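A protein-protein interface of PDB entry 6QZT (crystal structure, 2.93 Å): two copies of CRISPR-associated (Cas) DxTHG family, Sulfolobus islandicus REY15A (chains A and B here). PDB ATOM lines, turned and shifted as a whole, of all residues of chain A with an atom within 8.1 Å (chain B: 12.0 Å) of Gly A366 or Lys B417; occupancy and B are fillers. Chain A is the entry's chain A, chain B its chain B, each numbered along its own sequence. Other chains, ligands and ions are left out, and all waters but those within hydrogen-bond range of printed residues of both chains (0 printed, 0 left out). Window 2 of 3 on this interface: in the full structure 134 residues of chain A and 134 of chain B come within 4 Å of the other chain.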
ATOM      1  N   ASN A 328      -4.653  21.840 -15.767  1.00  0.00           N
ATOM      2  CA  ASN A 328      -4.252  22.237 -14.418  1.00  0.00           C
ATOM      3  C   ASN A 328      -3.159  23.275 -14.516  1.00  0.00           C
ATOM      4  O   ASN A 328      -2.485  23.350 -15.548  1.00  0.00           O
ATOM      5  CB  ASN A 328      -3.828  21.030 -13.549  1.00  0.00           C
ATOM      6  CG  ASN A 328      -2.565  20.275 -13.920  1.00  0.00           C
ATOM      7  OD1 ASN A 328      -1.746  20.702 -14.722  1.00  0.00           O
ATOM      8  ND2 ASN A 328      -2.367  19.119 -13.309  1.00  0.00           N
ATOM      9  N   LEU A 330      -0.185  23.385 -13.596  1.00  0.00           N
ATOM     10  CA  LEU A 330       1.092  22.799 -14.005  1.00  0.00           C
ATOM     11  C   LEU A 330       1.182  22.623 -15.530  1.00  0.00           C
ATOM     12  O   LEU A 330       2.239  22.862 -16.110  1.00  0.00           O
ATOM     13  CB  LEU A 330       1.284  21.463 -13.290  1.00  0.00           C
ATOM     14  CG  LEU A 330       2.359  21.388 -12.207  1.00  0.00           C
ATOM     15  CD1 LEU A 330       2.089  22.346 -11.082  1.00  0.00           C
ATOM     16  CD2 LEU A 330       2.411  20.018 -11.624  1.00  0.00           C
ATOM     17  N   ILE A 360       6.387  19.985 -10.371  1.00  0.00           N
ATOM     18  CA  ILE A 360       5.905  18.711 -10.923  1.00  0.00           C
ATOM     19  C   ILE A 360       6.146  17.628  -9.839  1.00  0.00           C
ATOM     20  O   ILE A 360       5.217  16.907  -9.454  1.00  0.00           O
ATOM     21  CB  ILE A 360       6.590  18.390 -12.296  1.00  0.00           C
ATOM     22  CG1 ILE A 360       6.077  19.309 -13.443  1.00  0.00           C
ATOM     23  CG2 ILE A 360       6.493  16.901 -12.671  1.00  0.00           C
ATOM     24  CD1 ILE A 360       4.823  18.808 -14.277  1.00  0.00           C
ATOM     25  N   CYS A 361       7.391  17.568  -9.318  1.00  0.00           N
ATOM     26  CA  CYS A 361       7.822  16.667  -8.249  1.00  0.00           C
ATOM     27  C   CYS A 361       6.903  16.847  -7.017  1.00  0.00           C
ATOM     28  O   CYS A 361       6.379  15.854  -6.511  1.00  0.00           O
ATOM     29  CB  CYS A 361       9.285  16.937  -7.900  1.00  0.00           C
ATOM     30  SG  CYS A 361       9.884  16.049  -6.439  1.00  0.00           S
ATOM     31  N   LEU A 362       6.691  18.120  -6.561  1.00  0.00           N
ATOM     32  CA  LEU A 362       5.852  18.469  -5.424  1.00  0.00           C
ATOM     33  C   LEU A 362       4.422  18.004  -5.603  1.00  0.00           C
ATOM     34  O   LEU A 362       3.805  17.670  -4.612  1.00  0.00           O
ATOM     35  CB  LEU A 362       5.907  19.964  -5.119  1.00  0.00           C
ATOM     36  CG  LEU A 362       6.903  20.427  -4.045  1.00  0.00           C
ATOM     37  CD1 LEU A 362       7.030  21.947  -4.033  1.00  0.00           C
ATOM     38  CD2 LEU A 362       6.466  20.000  -2.676  1.00  0.00           C
ATOM     39  N   ASN A 363       3.903  17.930  -6.845  1.00  0.00           N
ATOM     40  CA  ASN A 363       2.559  17.420  -7.126  1.00  0.00           C
ATOM     41  C   ASN A 363       2.536  15.906  -6.888  1.00  0.00           C
ATOM     42  O   ASN A 363       1.587  15.404  -6.276  1.00  0.00           O
ATOM     43  CB  ASN A 363       2.127  17.760  -8.560  1.00  0.00           C
ATOM     44  CG  ASN A 363       0.859  17.071  -9.035  1.00  0.00           C
ATOM     45  OD1 ASN A 363      -0.256  17.408  -8.623  1.00  0.00           O
ATOM     46  ND2 ASN A 363       1.000  16.079  -9.910  1.00  0.00           N
ATOM     47  N   LYS A 364       3.591  15.181  -7.347  1.00  0.00           N
ATOM     48  CA  LYS A 364       3.707  13.719  -7.195  1.00  0.00           C
ATOM     49  C   LYS A 364       3.694  13.305  -5.716  1.00  0.00           C
ATOM     50  O   LYS A 364       3.111  12.272  -5.369  1.00  0.00           O
ATOM     51  CB  LYS A 364       4.972  13.138  -7.883  1.00  0.00           C
ATOM     52  CG  LYS A 364       5.143  13.443  -9.368  1.00  0.00           C
ATOM     53  CD  LYS A 364       4.387  12.513 -10.302  1.00  0.00           C
ATOM     54  CE  LYS A 364       4.313  13.081 -11.710  1.00  0.00           C
ATOM     55  NZ  LYS A 364       3.522  14.350 -11.786  1.00  0.00           N
ATOM     56  N   VAL A 365       4.303  14.123  -4.846  1.00  0.00           N
ATOM     57  CA  VAL A 365       4.397  13.818  -3.424  1.00  0.00           C
ATOM     58  C   VAL A 365       3.213  14.399  -2.600  1.00  0.00           C
ATOM     59  O   VAL A 365       3.307  14.501  -1.375  1.00  0.00           O
ATOM     60  CB  VAL A 365       5.781  14.197  -2.845  1.00  0.00           C
ATOM     61  CG1 VAL A 365       6.886  13.418  -3.545  1.00  0.00           C
ATOM     62  CG2 VAL A 365       6.042  15.697  -2.930  1.00  0.00           C
ATOM     63  N   GLY A 366       2.105  14.717  -3.269  1.00  0.00           N
ATOM     64  CA  GLY A 366       0.897  15.209  -2.611  1.00  0.00           C
ATOM     65  C   GLY A 366       0.745  16.708  -2.457  1.00  0.00           C
ATOM     66  O   GLY A 366      -0.325  17.180  -2.060  1.00  0.00           O
ATOM     67  N   GLY A 367       1.809  17.449  -2.751  1.00  0.00           N
ATOM     68  CA  GLY A 367       1.802  18.905  -2.692  1.00  0.00           C
ATOM     69  C   GLY A 367       2.504  19.534  -1.511  1.00  0.00           C
ATOM     70  O   GLY A 367       2.645  18.913  -0.452  1.00  0.00           O
ATOM     71  N   GLY A 368       2.896  20.791  -1.708  1.00  0.00           N
ATOM     72  CA  GLY A 368       3.578  21.624  -0.727  1.00  0.00           C
ATOM     73  C   GLY A 368       3.934  23.010  -1.231  1.00  0.00           C
ATOM     74  O   GLY A 368       3.898  23.285  -2.435  1.00  0.00           O
ATOM     75  N   LYS A 376       8.883  18.410   1.664  1.00  0.00           N
ATOM     76  CA  LYS A 376       8.593  17.911   0.312  1.00  0.00           C
ATOM     77  C   LYS A 376       9.355  18.724  -0.742  1.00  0.00           C
ATOM     78  O   LYS A 376      10.028  18.128  -1.590  1.00  0.00           O
ATOM     79  CB  LYS A 376       7.076  17.863   0.033  1.00  0.00           C
ATOM     80  CG  LYS A 376       6.294  16.993   1.013  1.00  0.00           C
ATOM     81  CD  LYS A 376       4.887  16.711   0.544  1.00  0.00           C
ATOM     82  CE  LYS A 376       3.981  16.248   1.661  1.00  0.00           C
ATOM     83  NZ  LYS A 376       3.621  14.803   1.562  1.00  0.00           N
ATOM     84  N   CYS A 380      12.647  17.709  -3.177  1.00  0.00           N
ATOM     85  CA  CYS A 380      12.278  17.813  -4.590  1.00  0.00           C
ATOM     86  C   CYS A 380      13.314  18.669  -5.310  1.00  0.00           C
ATOM     87  O   CYS A 380      13.839  18.258  -6.348  1.00  0.00           O
ATOM     88  CB  CYS A 380      10.886  18.410  -4.746  1.00  0.00           C
ATOM     89  SG  CYS A 380       9.552  17.196  -4.776  1.00  0.00           S
ATOM     90  N   PRO B 413       4.693  30.027  -3.645  1.00  0.00           N
ATOM     91  CA  PRO B 413       3.369  29.542  -4.073  1.00  0.00           C
ATOM     92  C   PRO B 413       3.132  28.142  -3.519  1.00  0.00           C
ATOM     93  O   PRO B 413       4.089  27.501  -3.091  1.00  0.00           O
ATOM     94  CB  PRO B 413       3.487  29.512  -5.595  1.00  0.00           C
ATOM     95  CG  PRO B 413       4.920  29.289  -5.866  1.00  0.00           C
ATOM     96  CD  PRO B 413       5.665  29.980  -4.765  1.00  0.00           C
ATOM     97  N   ASN B 414       1.910  27.623  -3.548  1.00  0.00           N
ATOM     98  CA  ASN B 414       1.757  26.267  -3.018  1.00  0.00           C
ATOM     99  C   ASN B 414       1.064  25.269  -3.935  1.00  0.00           C
ATOM    100  O   ASN B 414      -0.087  25.446  -4.344  1.00  0.00           O
ATOM    101  CB  ASN B 414       1.206  26.257  -1.583  1.00  0.00           C
ATOM    102  CG  ASN B 414       0.149  27.299  -1.297  1.00  0.00           C
ATOM    103  OD1 ASN B 414      -1.046  27.071  -1.512  1.00  0.00           O
ATOM    104  ND2 ASN B 414       0.567  28.467  -0.811  1.00  0.00           N
ATOM    105  N   VAL B 415       1.813  24.243  -4.289  1.00  0.00           N
ATOM    106  CA  VAL B 415       1.312  23.146  -5.116  1.00  0.00           C
ATOM    107  C   VAL B 415       0.349  22.187  -4.368  1.00  0.00           C
ATOM    108  O   VAL B 415       0.578  21.916  -3.189  1.00  0.00           O
ATOM    109  CB  VAL B 415       2.503  22.394  -5.804  1.00  0.00           C
ATOM    110  CG1 VAL B 415       2.025  21.194  -6.620  1.00  0.00           C
ATOM    111  CG2 VAL B 415       3.391  23.314  -6.644  1.00  0.00           C
ATOM    112  N   ASP B 416      -0.745  21.735  -5.015  1.00  0.00           N
ATOM    113  CA  ASP B 416      -1.707  20.807  -4.401  1.00  0.00           C
ATOM    114  C   ASP B 416      -1.603  19.427  -5.104  1.00  0.00           C
ATOM    115  O   ASP B 416      -1.002  19.354  -6.183  1.00  0.00           O
ATOM    116  CB  ASP B 416      -3.169  21.295  -4.207  1.00  0.00           C
ATOM    117  CG  ASP B 416      -4.014  21.580  -5.438  1.00  0.00           C
ATOM    118  OD1 ASP B 416      -3.870  20.852  -6.443  1.00  0.00           O
ATOM    119  OD2 ASP B 416      -4.864  22.497  -5.372  1.00  0.00           O
ATOM    120  N   LYS B 417      -2.173  18.384  -4.492  1.00  0.00           N
ATOM    121  CA  LYS B 417      -2.128  17.014  -5.071  1.00  0.00           C
ATOM    122  C   LYS B 417      -2.739  17.043  -6.475  1.00  0.00           C
ATOM    123  O   LYS B 417      -2.215  16.345  -7.362  1.00  0.00           O
ATOM    124  CB  LYS B 417      -2.868  16.028  -4.162  1.00  0.00           C
ATOM    125  CG  LYS B 417      -2.841  14.577  -4.618  1.00  0.00           C
ATOM    126  CD  LYS B 417      -2.747  13.589  -3.474  1.00  0.00           C
ATOM    127  CE  LYS B 417      -2.349  12.198  -3.921  1.00  0.00           C
ATOM    128  NZ  LYS B 417      -1.080  11.761  -3.292  1.00  0.00           N
ATOM    129  N   ASP B 418      -3.810  17.823  -6.653  1.00  0.00           N
ATOM    130  CA  ASP B 418      -4.506  17.975  -7.960  1.00  0.00           C
ATOM    131  C   ASP B 418      -3.564  18.632  -8.976  1.00  0.00           C
ATOM    132  O   ASP B 418      -3.623  18.263 -10.163  1.00  0.00           O
ATOM    133  CB  ASP B 418      -5.838  18.713  -7.816  1.00  0.00           C
ATOM    134  CG  ASP B 418      -6.675  18.202  -6.658  1.00  0.00           C
ATOM    135  OD1 ASP B 418      -6.192  17.306  -5.941  1.00  0.00           O
ATOM    136  OD2 ASP B 418      -7.801  18.702  -6.487  1.00  0.00           O
ATOM    137  N   GLY B 419      -2.726  19.564  -8.512  1.00  0.00           N
ATOM    138  CA  GLY B 419      -1.788  20.292  -9.386  1.00  0.00           C
ATOM    139  C   GLY B 419      -2.151  21.760  -9.498  1.00  0.00           C
ATOM    140  O   GLY B 419      -1.423  22.494 -10.182  1.00  0.00           O
ATOM    141  N   ASN B 420      -3.241  22.176  -8.850  1.00  0.00           N
ATOM    142  CA  ASN B 420      -3.625  23.611  -8.848  1.00  0.00           C
ATOM    143  C   ASN B 420      -2.584  24.359  -8.008  1.00  0.00           C
ATOM    144  O   ASN B 420      -2.125  23.787  -7.005  1.00  0.00           O
ATOM    145  CB  ASN B 420      -5.042  23.819  -8.309  1.00  0.00           C
ATOM    146  CG  ASN B 420      -6.065  24.010  -9.407  1.00  0.00           C
ATOM    147  OD1 ASN B 420      -6.219  23.155 -10.275  1.00  0.00           O
ATOM    148  ND2 ASN B 420      -6.769  25.129  -9.379  1.00  0.00           N
ATOM    149  N   ILE B 421      -2.205  25.569  -8.432  1.00  0.00           N
ATOM    150  CA  ILE B 421      -1.181  26.370  -7.696  1.00  0.00           C
ATOM    151  C   ILE B 421      -1.776  27.735  -7.333  1.00  0.00           C
ATOM    152  O   ILE B 421      -2.451  28.336  -8.192  1.00  0.00           O
ATOM    153  CB  ILE B 421       0.109  26.517  -8.529  1.00  0.00           C
ATOM    154  CG1 ILE B 421       0.358  25.299  -9.422  1.00  0.00           C
ATOM    155  CG2 ILE B 421       1.300  26.810  -7.630  1.00  0.00           C
ATOM    156  CD1 ILE B 421       1.820  25.019  -9.685  1.00  0.00           C
ATOM    157  N   THR B 422      -1.524  28.196  -6.104  1.00  0.00           N
ATOM    158  CA  THR B 422      -2.029  29.513  -5.632  1.00  0.00           C
ATOM    159  C   THR B 422      -0.834  30.416  -5.306  1.00  0.00           C
ATOM    160  O   THR B 422       0.060  29.962  -4.565  1.00  0.00           O
ATOM    161  CB  THR B 422      -2.957  29.348  -4.422  1.00  0.00           C
ATOM    162  OG1 THR B 422      -2.212  28.729  -3.374  1.00  0.00           O
ATOM    163  CG2 THR B 422      -4.187  28.523  -4.731  1.00  0.00           C
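ND2 of Asn A328 lies within hydrogen-bond range of O of Asp B418 (3.5 Å).
O of Asp B416 lies close to OD1 of Asn A363, at 3.2 Å.
OD1 of Asn A363 lies close to O of Lys B417.
The side-chain amide oxygen of Asn A363 sits at hydrogen-bond distance from the backbone NH of Gly B419.
The backbone NH of Lys B417 sits at hydrogen-bond distance from the backbone carbonyl oxygen of Gly A366 (3.3 Å).
The backbone NH (N) of Val B415 is in hydrogen-bond range of the backbone carbonyl oxygen (O) of Gly A368 (2.9 Å).
No position is printed for both chains.
Of the 13 pairs that touch across the chains among the printed residues, none has its exchanged pair printed and touching as well.
Among the printed residues, merely in contact across the chains: Leu A330 with Gly B419, Leu A330 with Ile B421, Asn A363 with Val B415, Asn A363 with Asp B418, Gly A366 with Asp B416, Gly A367 with Val B415 and Gly A368 with Asn B414.
OD1 of Asn A328 lies close to N of Leu A330, 3.3 Å away.
O of Leu A362 sits at hydrogen-bond distance from N of Gly A367.
OD1 of Asn B414 lies within hydrogen-bond range of OG1 of Thr B422, at 2.8 Å.
The side-chain carboxylate (OD1) of Asp B416 sits at hydrogen-bond distance from the backbone NH (N) of Asp B418.
The side-chain carboxylate of Asp B416 lies within hydrogen-bond range of the backbone NH of Gly B419 (2.7 Å).
N of Asn B420 is in hydrogen-bond range of OD1 of Asp B416.
Of the 13 printed residues of chain A, 6 touch a printed residue of chain B.
Hydrophobic or aromatic side chains of chain A that line the printed part of chain B: Leu A330.
Among the printed residues, no Asp or Glu carboxylate lies within 4 Å of a Lys or Arg side-chain nitrogen of the other chain.
Of the printed residues of chain B, Gly A366 touches Asp B416 and Lys B417.
Of chain A, only Asn A363 (2.6 Å) and Gly A366 (3.3 Å) come within 4 Å of Lys B417.
Asn A363 touches five residues of chain B.
Val A365 touches none of the printed residues of chain B.
Gly A367 touches just one residue of chain B: Val B415 (3.3 Å).
Of chain B, only Asn B414 and Val B415 come within 4 Å of Gly A368.
Printed residues of chain A within 4 Å of Val B415: Asn A363 (3.8 Å), Gly A367 (3.3 Å) and Gly A368 (2.9 Å).
Printed residues of chain A within 4 Å of Gly B419: Leu A330 and Asn A363.
The nearest printed residue of chain B that does not touch Gly A366 is Val B415 (5.0 Å).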
